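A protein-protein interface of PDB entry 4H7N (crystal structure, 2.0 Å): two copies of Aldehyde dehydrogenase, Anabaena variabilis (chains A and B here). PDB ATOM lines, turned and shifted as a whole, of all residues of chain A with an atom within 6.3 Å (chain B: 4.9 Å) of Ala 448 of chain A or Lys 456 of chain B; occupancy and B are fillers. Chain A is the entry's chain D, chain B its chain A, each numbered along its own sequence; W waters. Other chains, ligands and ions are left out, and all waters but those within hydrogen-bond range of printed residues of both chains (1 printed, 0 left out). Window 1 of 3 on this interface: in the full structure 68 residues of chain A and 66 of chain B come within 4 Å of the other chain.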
ATOM      1  N   LEU A 105      25.215  -9.533 -28.266  1.00  0.00           N
ATOM      2  CA  LEU A 105      23.929  -9.327 -28.880  1.00  0.00           C
ATOM      3  C   LEU A 105      23.801  -9.867 -30.315  1.00  0.00           C
ATOM      4  O   LEU A 105      22.709 -10.235 -30.747  1.00  0.00           O
ATOM      5  CB  LEU A 105      23.577  -7.823 -28.860  1.00  0.00           C
ATOM      6  CG  LEU A 105      23.287  -7.283 -27.464  1.00  0.00           C
ATOM      7  CD1 LEU A 105      22.892  -5.826 -27.617  1.00  0.00           C
ATOM      8  CD2 LEU A 105      22.170  -8.100 -26.848  1.00  0.00           C
ATOM      9  N   ALA A 413       2.445   5.456 -19.175  1.00  0.00           N
ATOM     10  CA  ALA A 413       3.697   6.033 -19.658  1.00  0.00           C
ATOM     11  C   ALA A 413       4.780   4.991 -19.594  1.00  0.00           C
ATOM     12  O   ALA A 413       4.721   4.125 -18.753  1.00  0.00           O
ATOM     13  CB  ALA A 413       4.074   7.255 -18.828  1.00  0.00           C
ATOM     14  N   GLY A 414       5.782   5.123 -20.455  1.00  0.00           N
ATOM     15  CA  GLY A 414       6.880   4.166 -20.546  1.00  0.00           C
ATOM     16  C   GLY A 414       7.918   4.161 -19.436  1.00  0.00           C
ATOM     17  O   GLY A 414       8.402   3.096 -19.028  1.00  0.00           O
ATOM     18  N   ALA A 415       8.303   5.325 -18.938  1.00  0.00           N
ATOM     19  CA  ALA A 415       9.339   5.351 -17.889  1.00  0.00           C
ATOM     20  C   ALA A 415       8.877   6.282 -16.766  1.00  0.00           C
ATOM     21  O   ALA A 415       8.617   7.436 -17.011  1.00  0.00           O
ATOM     22  CB  ALA A 415      10.682   5.810 -18.471  1.00  0.00           C
ATOM     23  N   GLU A 431      14.142  -0.634 -20.147  1.00  0.00           N
ATOM     24  CA  GLU A 431      13.439  -0.881 -21.396  1.00  0.00           C
ATOM     25  C   GLU A 431      12.076  -0.239 -21.288  1.00  0.00           C
ATOM     26  O   GLU A 431      11.372  -0.428 -20.284  1.00  0.00           O
ATOM     27  CB  GLU A 431      13.195  -2.360 -21.564  1.00  0.00           C
ATOM     28  CG  GLU A 431      14.416  -3.191 -21.800  1.00  0.00           C
ATOM     29  CD  GLU A 431      13.981  -4.509 -22.366  1.00  0.00           C
ATOM     30  OE1 GLU A 431      13.743  -5.420 -21.527  1.00  0.00           O
ATOM     31  OE2 GLU A 431      13.798  -4.567 -23.618  1.00  0.00           O
ATOM     32  N   LYS A 432      11.702   0.530 -22.294  1.00  0.00           N
ATOM     33  CA  LYS A 432      10.446   1.252 -22.242  1.00  0.00           C
ATOM     34  C   LYS A 432       9.817   1.355 -23.624  1.00  0.00           C
ATOM     35  O   LYS A 432      10.515   1.457 -24.626  1.00  0.00           O
ATOM     36  CB  LYS A 432      10.628   2.637 -21.622  1.00  0.00           C
ATOM     37  CG  LYS A 432      11.736   3.467 -22.234  1.00  0.00           C
ATOM     38  CD  LYS A 432      12.569   4.171 -21.171  1.00  0.00           C
ATOM     39  CE  LYS A 432      13.810   4.843 -21.762  1.00  0.00           C
ATOM     40  NZ  LYS A 432      15.011   4.368 -21.030  1.00  0.00           N
ATOM     41  N   ASN A 433       8.498   1.263 -23.645  1.00  0.00           N
ATOM     42  CA  ASN A 433       7.672   1.565 -24.816  1.00  0.00           C
ATOM     43  C   ASN A 433       6.842   2.823 -24.539  1.00  0.00           C
ATOM     44  O   ASN A 433       6.203   2.960 -23.491  1.00  0.00           O
ATOM     45  CB  ASN A 433       6.754   0.366 -25.176  1.00  0.00           C
ATOM     46  CG  ASN A 433       7.552  -0.865 -25.550  1.00  0.00           C
ATOM     47  OD1 ASN A 433       7.303  -1.945 -25.084  1.00  0.00           O
ATOM     48  ND2 ASN A 433       8.604  -0.662 -26.322  1.00  0.00           N
ATOM     49  N   ALA A 434       6.863   3.751 -25.476  1.00  0.00           N
ATOM     50  CA  ALA A 434       5.974   4.919 -25.430  1.00  0.00           C
ATOM     51  C   ALA A 434       4.494   4.504 -25.442  1.00  0.00           C
ATOM     52  O   ALA A 434       4.116   3.590 -26.137  1.00  0.00           O
ATOM     53  CB  ALA A 434       6.259   5.792 -26.622  1.00  0.00           C
ATOM     54  N   PHE A 435       3.661   5.214 -24.705  1.00  0.00           N
ATOM     55  CA  PHE A 435       2.219   5.056 -24.810  1.00  0.00           C
ATOM     56  C   PHE A 435       1.585   6.207 -25.622  1.00  0.00           C
ATOM     57  O   PHE A 435       2.167   7.304 -25.777  1.00  0.00           O
ATOM     58  CB  PHE A 435       1.611   5.088 -23.420  1.00  0.00           C
ATOM     59  CG  PHE A 435       1.888   3.866 -22.576  1.00  0.00           C
ATOM     60  CD1 PHE A 435       3.183   3.484 -22.260  1.00  0.00           C
ATOM     61  CD2 PHE A 435       0.827   3.125 -22.067  1.00  0.00           C
ATOM     62  CE1 PHE A 435       3.417   2.372 -21.452  1.00  0.00           C
ATOM     63  CE2 PHE A 435       1.050   2.012 -21.248  1.00  0.00           C
ATOM     64  CZ  PHE A 435       2.345   1.649 -20.925  1.00  0.00           C
ATOM     65  N   SER A 443      11.646  -0.243 -28.234  1.00  0.00           N
ATOM     66  CA  SER A 443      12.535   0.380 -27.240  1.00  0.00           C
ATOM     67  C   SER A 443      13.935   0.507 -27.801  1.00  0.00           C
ATOM     68  O   SER A 443      14.302  -0.270 -28.683  1.00  0.00           O
ATOM     69  CB  SER A 443      12.603  -0.488 -25.994  1.00  0.00           C
ATOM     70  OG  SER A 443      13.387   0.196 -24.989  1.00  0.00           O
ATOM     71  N   ARG A 444      14.736   1.431 -27.259  1.00  0.00           N
ATOM     72  CA  ARG A 444      16.153   1.553 -27.640  1.00  0.00           C
ATOM     73  C   ARG A 444      17.163   0.778 -26.805  1.00  0.00           C
ATOM     74  O   ARG A 444      18.325   0.682 -27.229  1.00  0.00           O
ATOM     75  CB  ARG A 444      16.611   2.979 -27.591  1.00  0.00           C
ATOM     76  CG  ARG A 444      15.929   3.847 -28.596  1.00  0.00           C
ATOM     77  CD  ARG A 444      16.322   5.286 -28.355  1.00  0.00           C
ATOM     78  NE  ARG A 444      16.004   6.050 -29.551  1.00  0.00           N
ATOM     79  CZ  ARG A 444      15.540   7.279 -29.577  1.00  0.00           C
ATOM     80  NH1 ARG A 444      15.273   7.848 -30.734  1.00  0.00           N
ATOM     81  NH2 ARG A 444      15.345   7.935 -28.456  1.00  0.00           N
ATOM     82  N   VAL A 445      16.778   0.256 -25.639  1.00  0.00           N
ATOM     83  CA  VAL A 445      17.765  -0.293 -24.749  1.00  0.00           C
ATOM     84  C   VAL A 445      18.070  -1.777 -25.019  1.00  0.00           C
ATOM     85  O   VAL A 445      17.178  -2.580 -25.288  1.00  0.00           O
ATOM     86  CB  VAL A 445      17.330  -0.080 -23.303  1.00  0.00           C
ATOM     87  CG1 VAL A 445      18.350  -0.717 -22.366  1.00  0.00           C
ATOM     88  CG2 VAL A 445      17.143   1.415 -23.039  1.00  0.00           C
ATOM     89  N   GLY A 446      19.350  -2.121 -24.974  1.00  0.00           N
ATOM     90  CA  GLY A 446      19.773  -3.509 -24.913  1.00  0.00           C
ATOM     91  C   GLY A 446      19.470  -4.327 -26.141  1.00  0.00           C
ATOM     92  O   GLY A 446      19.449  -3.818 -27.269  1.00  0.00           O
ATOM     93  N   ALA A 447      19.200  -5.601 -25.925  1.00  0.00           N
ATOM     94  CA  ALA A 447      18.924  -6.513 -27.014  1.00  0.00           C
ATOM     95  C   ALA A 447      17.905  -5.938 -27.987  1.00  0.00           C
ATOM     96  O   ALA A 447      18.145  -5.924 -29.184  1.00  0.00           O
ATOM     97  CB  ALA A 447      18.456  -7.866 -26.483  1.00  0.00           C
ATOM     98  N   ALA A 448      16.788  -5.442 -27.457  1.00  0.00           N
ATOM     99  CA  ALA A 448      15.657  -4.997 -28.265  1.00  0.00           C
ATOM    100  C   ALA A 448      15.997  -3.751 -29.062  1.00  0.00           C
ATOM    101  O   ALA A 448      15.530  -3.586 -30.180  1.00  0.00           O
ATOM    102  CB  ALA A 448      14.437  -4.741 -27.378  1.00  0.00           C
ATOM    103  N   GLY A 449      16.822  -2.887 -28.495  1.00  0.00           N
ATOM    104  CA  GLY A 449      17.249  -1.670 -29.143  1.00  0.00           C
ATOM    105  C   GLY A 449      18.252  -1.782 -30.282  1.00  0.00           C
ATOM    106  O   GLY A 449      18.287  -0.932 -31.176  1.00  0.00           O
ATOM    107  N   LEU A 450      19.143  -2.758 -30.214  1.00  0.00           N
ATOM    108  CA  LEU A 450      20.050  -3.017 -31.316  1.00  0.00           C
ATOM    109  C   LEU A 450      19.369  -3.941 -32.259  1.00  0.00           C
ATOM    110  O   LEU A 450      19.516  -3.762 -33.445  1.00  0.00           O
ATOM    111  CB  LEU A 450      21.350  -3.645 -30.869  1.00  0.00           C
ATOM    112  CG  LEU A 450      22.384  -3.686 -31.997  1.00  0.00           C
ATOM    113  CD1 LEU A 450      23.734  -3.164 -31.550  1.00  0.00           C
ATOM    114  CD2 LEU A 450      22.490  -5.116 -32.417  1.00  0.00           C
ATOM    115  N   LYS A 451      18.557  -4.882 -31.764  1.00  0.00           N
ATOM    116  CA  LYS A 451      17.917  -5.846 -32.684  1.00  0.00           C
ATOM    117  C   LYS A 451      16.794  -5.307 -33.495  1.00  0.00           C
ATOM    118  O   LYS A 451      16.414  -5.926 -34.486  1.00  0.00           O
ATOM    119  CB  LYS A 451      17.492  -7.134 -31.971  1.00  0.00           C
ATOM    120  CG  LYS A 451      18.673  -8.031 -31.591  1.00  0.00           C
ATOM    121  CD  LYS A 451      18.214  -9.428 -31.211  1.00  0.00           C
ATOM    122  CE  LYS A 451      19.287 -10.149 -30.409  1.00  0.00           C
ATOM    123  NZ  LYS A 451      18.764 -11.476 -30.007  1.00  0.00           N
ATOM    124  N   ARG A 452      16.281  -4.121 -33.172  1.00  0.00           N
ATOM    125  CA  ARG A 452      15.384  -3.424 -34.088  1.00  0.00           C
ATOM    126  C   ARG A 452      15.960  -3.386 -35.488  1.00  0.00           C
ATOM    127  O   ARG A 452      15.206  -3.322 -36.478  1.00  0.00           O
ATOM    128  CB  ARG A 452      15.261  -1.922 -33.710  1.00  0.00           C
ATOM    129  CG  ARG A 452      14.512  -1.556 -32.490  1.00  0.00           C
ATOM    130  CD  ARG A 452      14.578  -0.028 -32.269  1.00  0.00           C
ATOM    131  NE  ARG A 452      15.887   0.479 -31.845  1.00  0.00           N
ATOM    132  CZ  ARG A 452      16.233   1.767 -31.878  1.00  0.00           C
ATOM    133  NH1 ARG A 452      15.395   2.680 -32.306  1.00  0.00           N
ATOM    134  NH2 ARG A 452      17.432   2.169 -31.491  1.00  0.00           N
ATOM    135  N   PHE A 453      17.296  -3.289 -35.597  1.00  0.00           N
ATOM    136  CA  PHE A 453      17.915  -3.028 -36.889  1.00  0.00           C
ATOM    137  C   PHE A 453      18.350  -4.286 -37.651  1.00  0.00           C
ATOM    138  O   PHE A 453      19.082  -4.175 -38.634  1.00  0.00           O
ATOM    139  CB  PHE A 453      19.138  -2.086 -36.724  1.00  0.00           C
ATOM    140  CG  PHE A 453      18.789  -0.785 -36.106  1.00  0.00           C
ATOM    141  CD1 PHE A 453      17.983   0.061 -36.754  1.00  0.00           C
ATOM    142  CD2 PHE A 453      19.253  -0.447 -34.850  1.00  0.00           C
ATOM    143  CE1 PHE A 453      17.622   1.242 -36.206  1.00  0.00           C
ATOM    144  CE2 PHE A 453      18.924   0.755 -34.284  1.00  0.00           C
ATOM    145  CZ  PHE A 453      18.093   1.602 -34.963  1.00  0.00           C
ATOM    146  N   GLN B 122      11.120  -3.392 -13.750  1.00  0.00           N
ATOM    147  CA  GLN B 122      10.469  -3.460 -15.061  1.00  0.00           C
ATOM    148  C   GLN B 122       9.097  -4.108 -14.918  1.00  0.00           C
ATOM    149  O   GLN B 122       8.913  -4.979 -14.077  1.00  0.00           O
ATOM    150  CB  GLN B 122      11.309  -4.282 -16.020  1.00  0.00           C
ATOM    151  CG  GLN B 122      12.730  -3.753 -16.287  1.00  0.00           C
ATOM    152  CD  GLN B 122      12.815  -2.694 -17.430  1.00  0.00           C
ATOM    153  OE1 GLN B 122      13.906  -2.241 -17.793  1.00  0.00           O
ATOM    154  NE2 GLN B 122      11.669  -2.307 -17.983  1.00  0.00           N
ATOM    155  N   SER B 123       8.119  -3.657 -15.703  1.00  0.00           N
ATOM    156  CA  SER B 123       6.851  -4.411 -15.822  1.00  0.00           C
ATOM    157  C   SER B 123       6.313  -4.320 -17.228  1.00  0.00           C
ATOM    158  O   SER B 123       6.893  -3.641 -18.074  1.00  0.00           O
ATOM    159  CB  SER B 123       5.790  -3.959 -14.813  1.00  0.00           C
ATOM    160  OG  SER B 123       5.321  -2.676 -15.156  1.00  0.00           O
ATOM    161  N   LEU B 124       5.232  -5.052 -17.481  1.00  0.00           N
ATOM    162  CA  LEU B 124       4.679  -5.201 -18.808  1.00  0.00           C
ATOM    163  C   LEU B 124       3.161  -4.937 -18.787  1.00  0.00           C
ATOM    164  O   LEU B 124       2.463  -5.498 -17.977  1.00  0.00           O
ATOM    165  CB  LEU B 124       4.973  -6.602 -19.279  1.00  0.00           C
ATOM    166  CG  LEU B 124       6.478  -6.856 -19.361  1.00  0.00           C
ATOM    167  CD1 LEU B 124       6.802  -8.228 -18.774  1.00  0.00           C
ATOM    168  CD2 LEU B 124       6.995  -6.703 -20.768  1.00  0.00           C
ATOM    169  N   LYS B 451       5.521 -11.025 -26.574  1.00  0.00           N
ATOM    170  CA  LYS B 451       5.913  -9.714 -26.123  1.00  0.00           C
ATOM    171  C   LYS B 451       5.500  -8.569 -27.013  1.00  0.00           C
ATOM    172  O   LYS B 451       5.317  -7.450 -26.565  1.00  0.00           O
ATOM    173  CB  LYS B 451       7.400  -9.713 -25.850  1.00  0.00           C
ATOM    174  CG  LYS B 451       7.729 -10.623 -24.668  1.00  0.00           C
ATOM    175  CD  LYS B 451       9.210 -10.593 -24.299  1.00  0.00           C
ATOM    176  CE  LYS B 451       9.476  -9.562 -23.204  1.00  0.00           C
ATOM    177  NZ  LYS B 451       8.821  -9.985 -21.933  1.00  0.00           N
ATOM    178  N   LEU B 454       2.632  -6.409 -25.431  1.00  0.00           N
ATOM    179  CA  LEU B 454       2.931  -5.787 -24.129  1.00  0.00           C
ATOM    180  C   LEU B 454       3.763  -4.563 -24.323  1.00  0.00           C
ATOM    181  O   LEU B 454       4.636  -4.539 -25.225  1.00  0.00           O
ATOM    182  CB  LEU B 454       3.734  -6.773 -23.265  1.00  0.00           C
ATOM    183  CG  LEU B 454       2.911  -8.036 -22.898  1.00  0.00           C
ATOM    184  CD1 LEU B 454       3.892  -9.119 -22.531  1.00  0.00           C
ATOM    185  CD2 LEU B 454       1.982  -7.751 -21.728  1.00  0.00           C
ATOM    186  N   ARG B 455       3.465  -3.516 -23.566  1.00  0.00           N
ATOM    187  CA  ARG B 455       4.351  -2.381 -23.529  1.00  0.00           C
ATOM    188  C   ARG B 455       5.205  -2.549 -22.276  1.00  0.00           C
ATOM    189  O   ARG B 455       4.701  -2.860 -21.210  1.00  0.00           O
ATOM    190  CB  ARG B 455       3.586  -1.083 -23.428  1.00  0.00           C
ATOM    191  CG  ARG B 455       2.883  -0.688 -24.693  1.00  0.00           C
ATOM    192  CD  ARG B 455       2.433   0.754 -24.508  1.00  0.00           C
ATOM    193  NE  ARG B 455       1.783   1.358 -25.683  1.00  0.00           N
ATOM    194  CZ  ARG B 455       0.480   1.322 -25.937  1.00  0.00           C
ATOM    195  NH1 ARG B 455       0.020   1.951 -27.021  1.00  0.00           N
ATOM    196  NH2 ARG B 455      -0.352   0.654 -25.140  1.00  0.00           N
ATOM    197  N   LYS B 456       6.494  -2.359 -22.442  1.00  0.00           N
ATOM    198  CA  LYS B 456       7.437  -2.371 -21.345  1.00  0.00           C
ATOM    199  C   LYS B 456       7.413  -1.035 -20.647  1.00  0.00           C
ATOM    200  O   LYS B 456       7.351   0.017 -21.289  1.00  0.00           O
ATOM    201  CB  LYS B 456       8.843  -2.672 -21.894  1.00  0.00           C
ATOM    202  CG  LYS B 456       9.011  -4.093 -22.407  1.00  0.00           C
ATOM    203  CD  LYS B 456      10.345  -4.252 -23.140  1.00  0.00           C
ATOM    204  CE  LYS B 456      10.288  -5.276 -24.281  1.00  0.00           C
ATOM    205  NZ  LYS B 456      11.554  -5.146 -25.083  1.00  0.00           N
ATOM    206  N   GLN B 457       7.417  -1.082 -19.329  1.00  0.00           N
ATOM    207  CA  GLN B 457       7.469   0.102 -18.465  1.00  0.00           C
ATOM    208  C   GLN B 457       8.661  -0.017 -17.564  1.00  0.00           C
ATOM    209  O   GLN B 457       8.861  -1.061 -16.939  1.00  0.00           O
ATOM    210  CB  GLN B 457       6.261   0.120 -17.537  1.00  0.00           C
ATOM    211  CG  GLN B 457       5.049   0.752 -18.066  1.00  0.00           C
ATOM    212  CD  GLN B 457       3.999   0.988 -16.977  1.00  0.00           C
ATOM    213  OE1 GLN B 457       3.714   0.113 -16.167  1.00  0.00           O
ATOM    214  NE2 GLN B 457       3.413   2.154 -16.990  1.00  0.00           N
ATOM    215  N   ALA B 458       9.470   1.026 -17.486  1.00  0.00           N
ATOM    216  CA  ALA B 458      10.595   1.061 -16.543  1.00  0.00           C
ATOM    217  C   ALA B 458      10.257   1.986 -15.361  1.00  0.00           C
ATOM    218  O   ALA B 458       9.600   3.025 -15.528  1.00  0.00           O
ATOM    219  CB  ALA B 458      11.850   1.532 -17.257  1.00  0.00           C
HETATM  220  O   HOH W   1      10.892  -3.249 -27.259  1.00  0.00           O
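The side-chain amide oxygen of Gln 122 of chain B lies within hydrogen-bond range of the backbone NH of Glu 431 of chain A, at 2.9 Å. The guanidinium group of Arg 455 of chain B is in hydrogen-bond range of the backbone carbonyl oxygen of Ala 434 of chain A (3.3 Å). The side-chain carboxylate of Glu 431 of chain A lies within salt-bridge range of the side-chain amino group of Lys 456 of chain B (2.7 Å). N of Lys 456 of chain B sits at hydrogen-bond distance from OD1 of Asn 433 of chain A (2.8 Å). The side-chain amide nitrogen (NE2) of Gln 457 of chain B is in hydrogen-bond range of the backbone carbonyl oxygen (O) of Ala 413 of chain A (3.0 Å). N of Ala 458 of chain B is in hydrogen-bond range of O of Gly 414 of chain A (2.8 Å).
O of Gln 457 of chain B lies within hydrogen-bond range of NE2 of Gln 122 of chain B (3.2 Å). N of Gln 457 of chain B sits at hydrogen-bond distance from O of Ser 123 of chain B, 2.9 Å away. The side-chain hydroxyl (OG) of Ser 443 of chain A lies within hydrogen-bond range of the backbone carbonyl oxygen (O) of Lys 432 of chain A (3.2 Å).
Among the printed residues, pairs that only touch across the chains: Gly 414 of chain A with Gln 457 of chain B (3.2 Å), Ala 415 of chain A with Ala 458 of chain B (3.3 Å), Asn 433 of chain A with Arg 455 of chain B (3.4 Å), Lys 432 of chain A with Lys 456 of chain B (3.5 Å), Phe 435 of chain A with Arg 455 of chain B (3.6 Å), Glu 431 of chain A with Ala 458 of chain B (3.6 Å), Ala 448 of chain A with Lys 456 of chain B (3.7 Å), Asn 433 of chain A with Leu 454 of chain B (3.7 Å), Glu 431 of chain A with Gln 457 of chain B (3.9 Å) and Gly 414 of chain A with Lys 456 of chain B (3.96 Å).
Printed residues of chain B within 4 Å of Glu 431 of chain A: Gln 122, Lys 456, Gln 457 and Ala 458. Of the printed residues of chain B, Ala 434 of chain A touches Arg 455. Arg 444 of chain A touches none of the printed residues of chain B. Gly 446 of chain A touches none of the printed residues of chain B. Of chain B, only Lys 456 (3.7 Å) comes within 4 Å of Ala 448 of chain A. Of the printed residues of chain A, Lys 456 of chain B touches Gly 414 (3.96 Å), Glu 431 (2.7 Å), Lys 432 (3.5 Å), Asn 433 (2.8 Å) and Ala 448 (3.7 Å). Of the printed residues of chain A, Gln 457 of chain B touches Ala 413, Gly 414 and Glu 431.
Of the 20 printed residues of chain A, 9 touch a printed residue of chain B. Hydrophobic or aromatic side chains of chain A within 4 Å of the printed part of chain B: Phe 435 and Ala 448. Among the printed residues, Asp or Glu carboxylates within 4 Å of a Lys or Arg side-chain nitrogen of the other chain: Glu 431 of chain A with Lys 456 of chain B.
1 position is printed for both chains. Of the 16 pairs that touch across the chains among the printed residues, none has its exchanged pair printed and touching as well.
Water W1 lies within hydrogen-bond range of the side-chain amino group of Lys 456 of chain B (3.0 Å) and the backbone NH of Ser 443 of chain A (3.2 Å).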
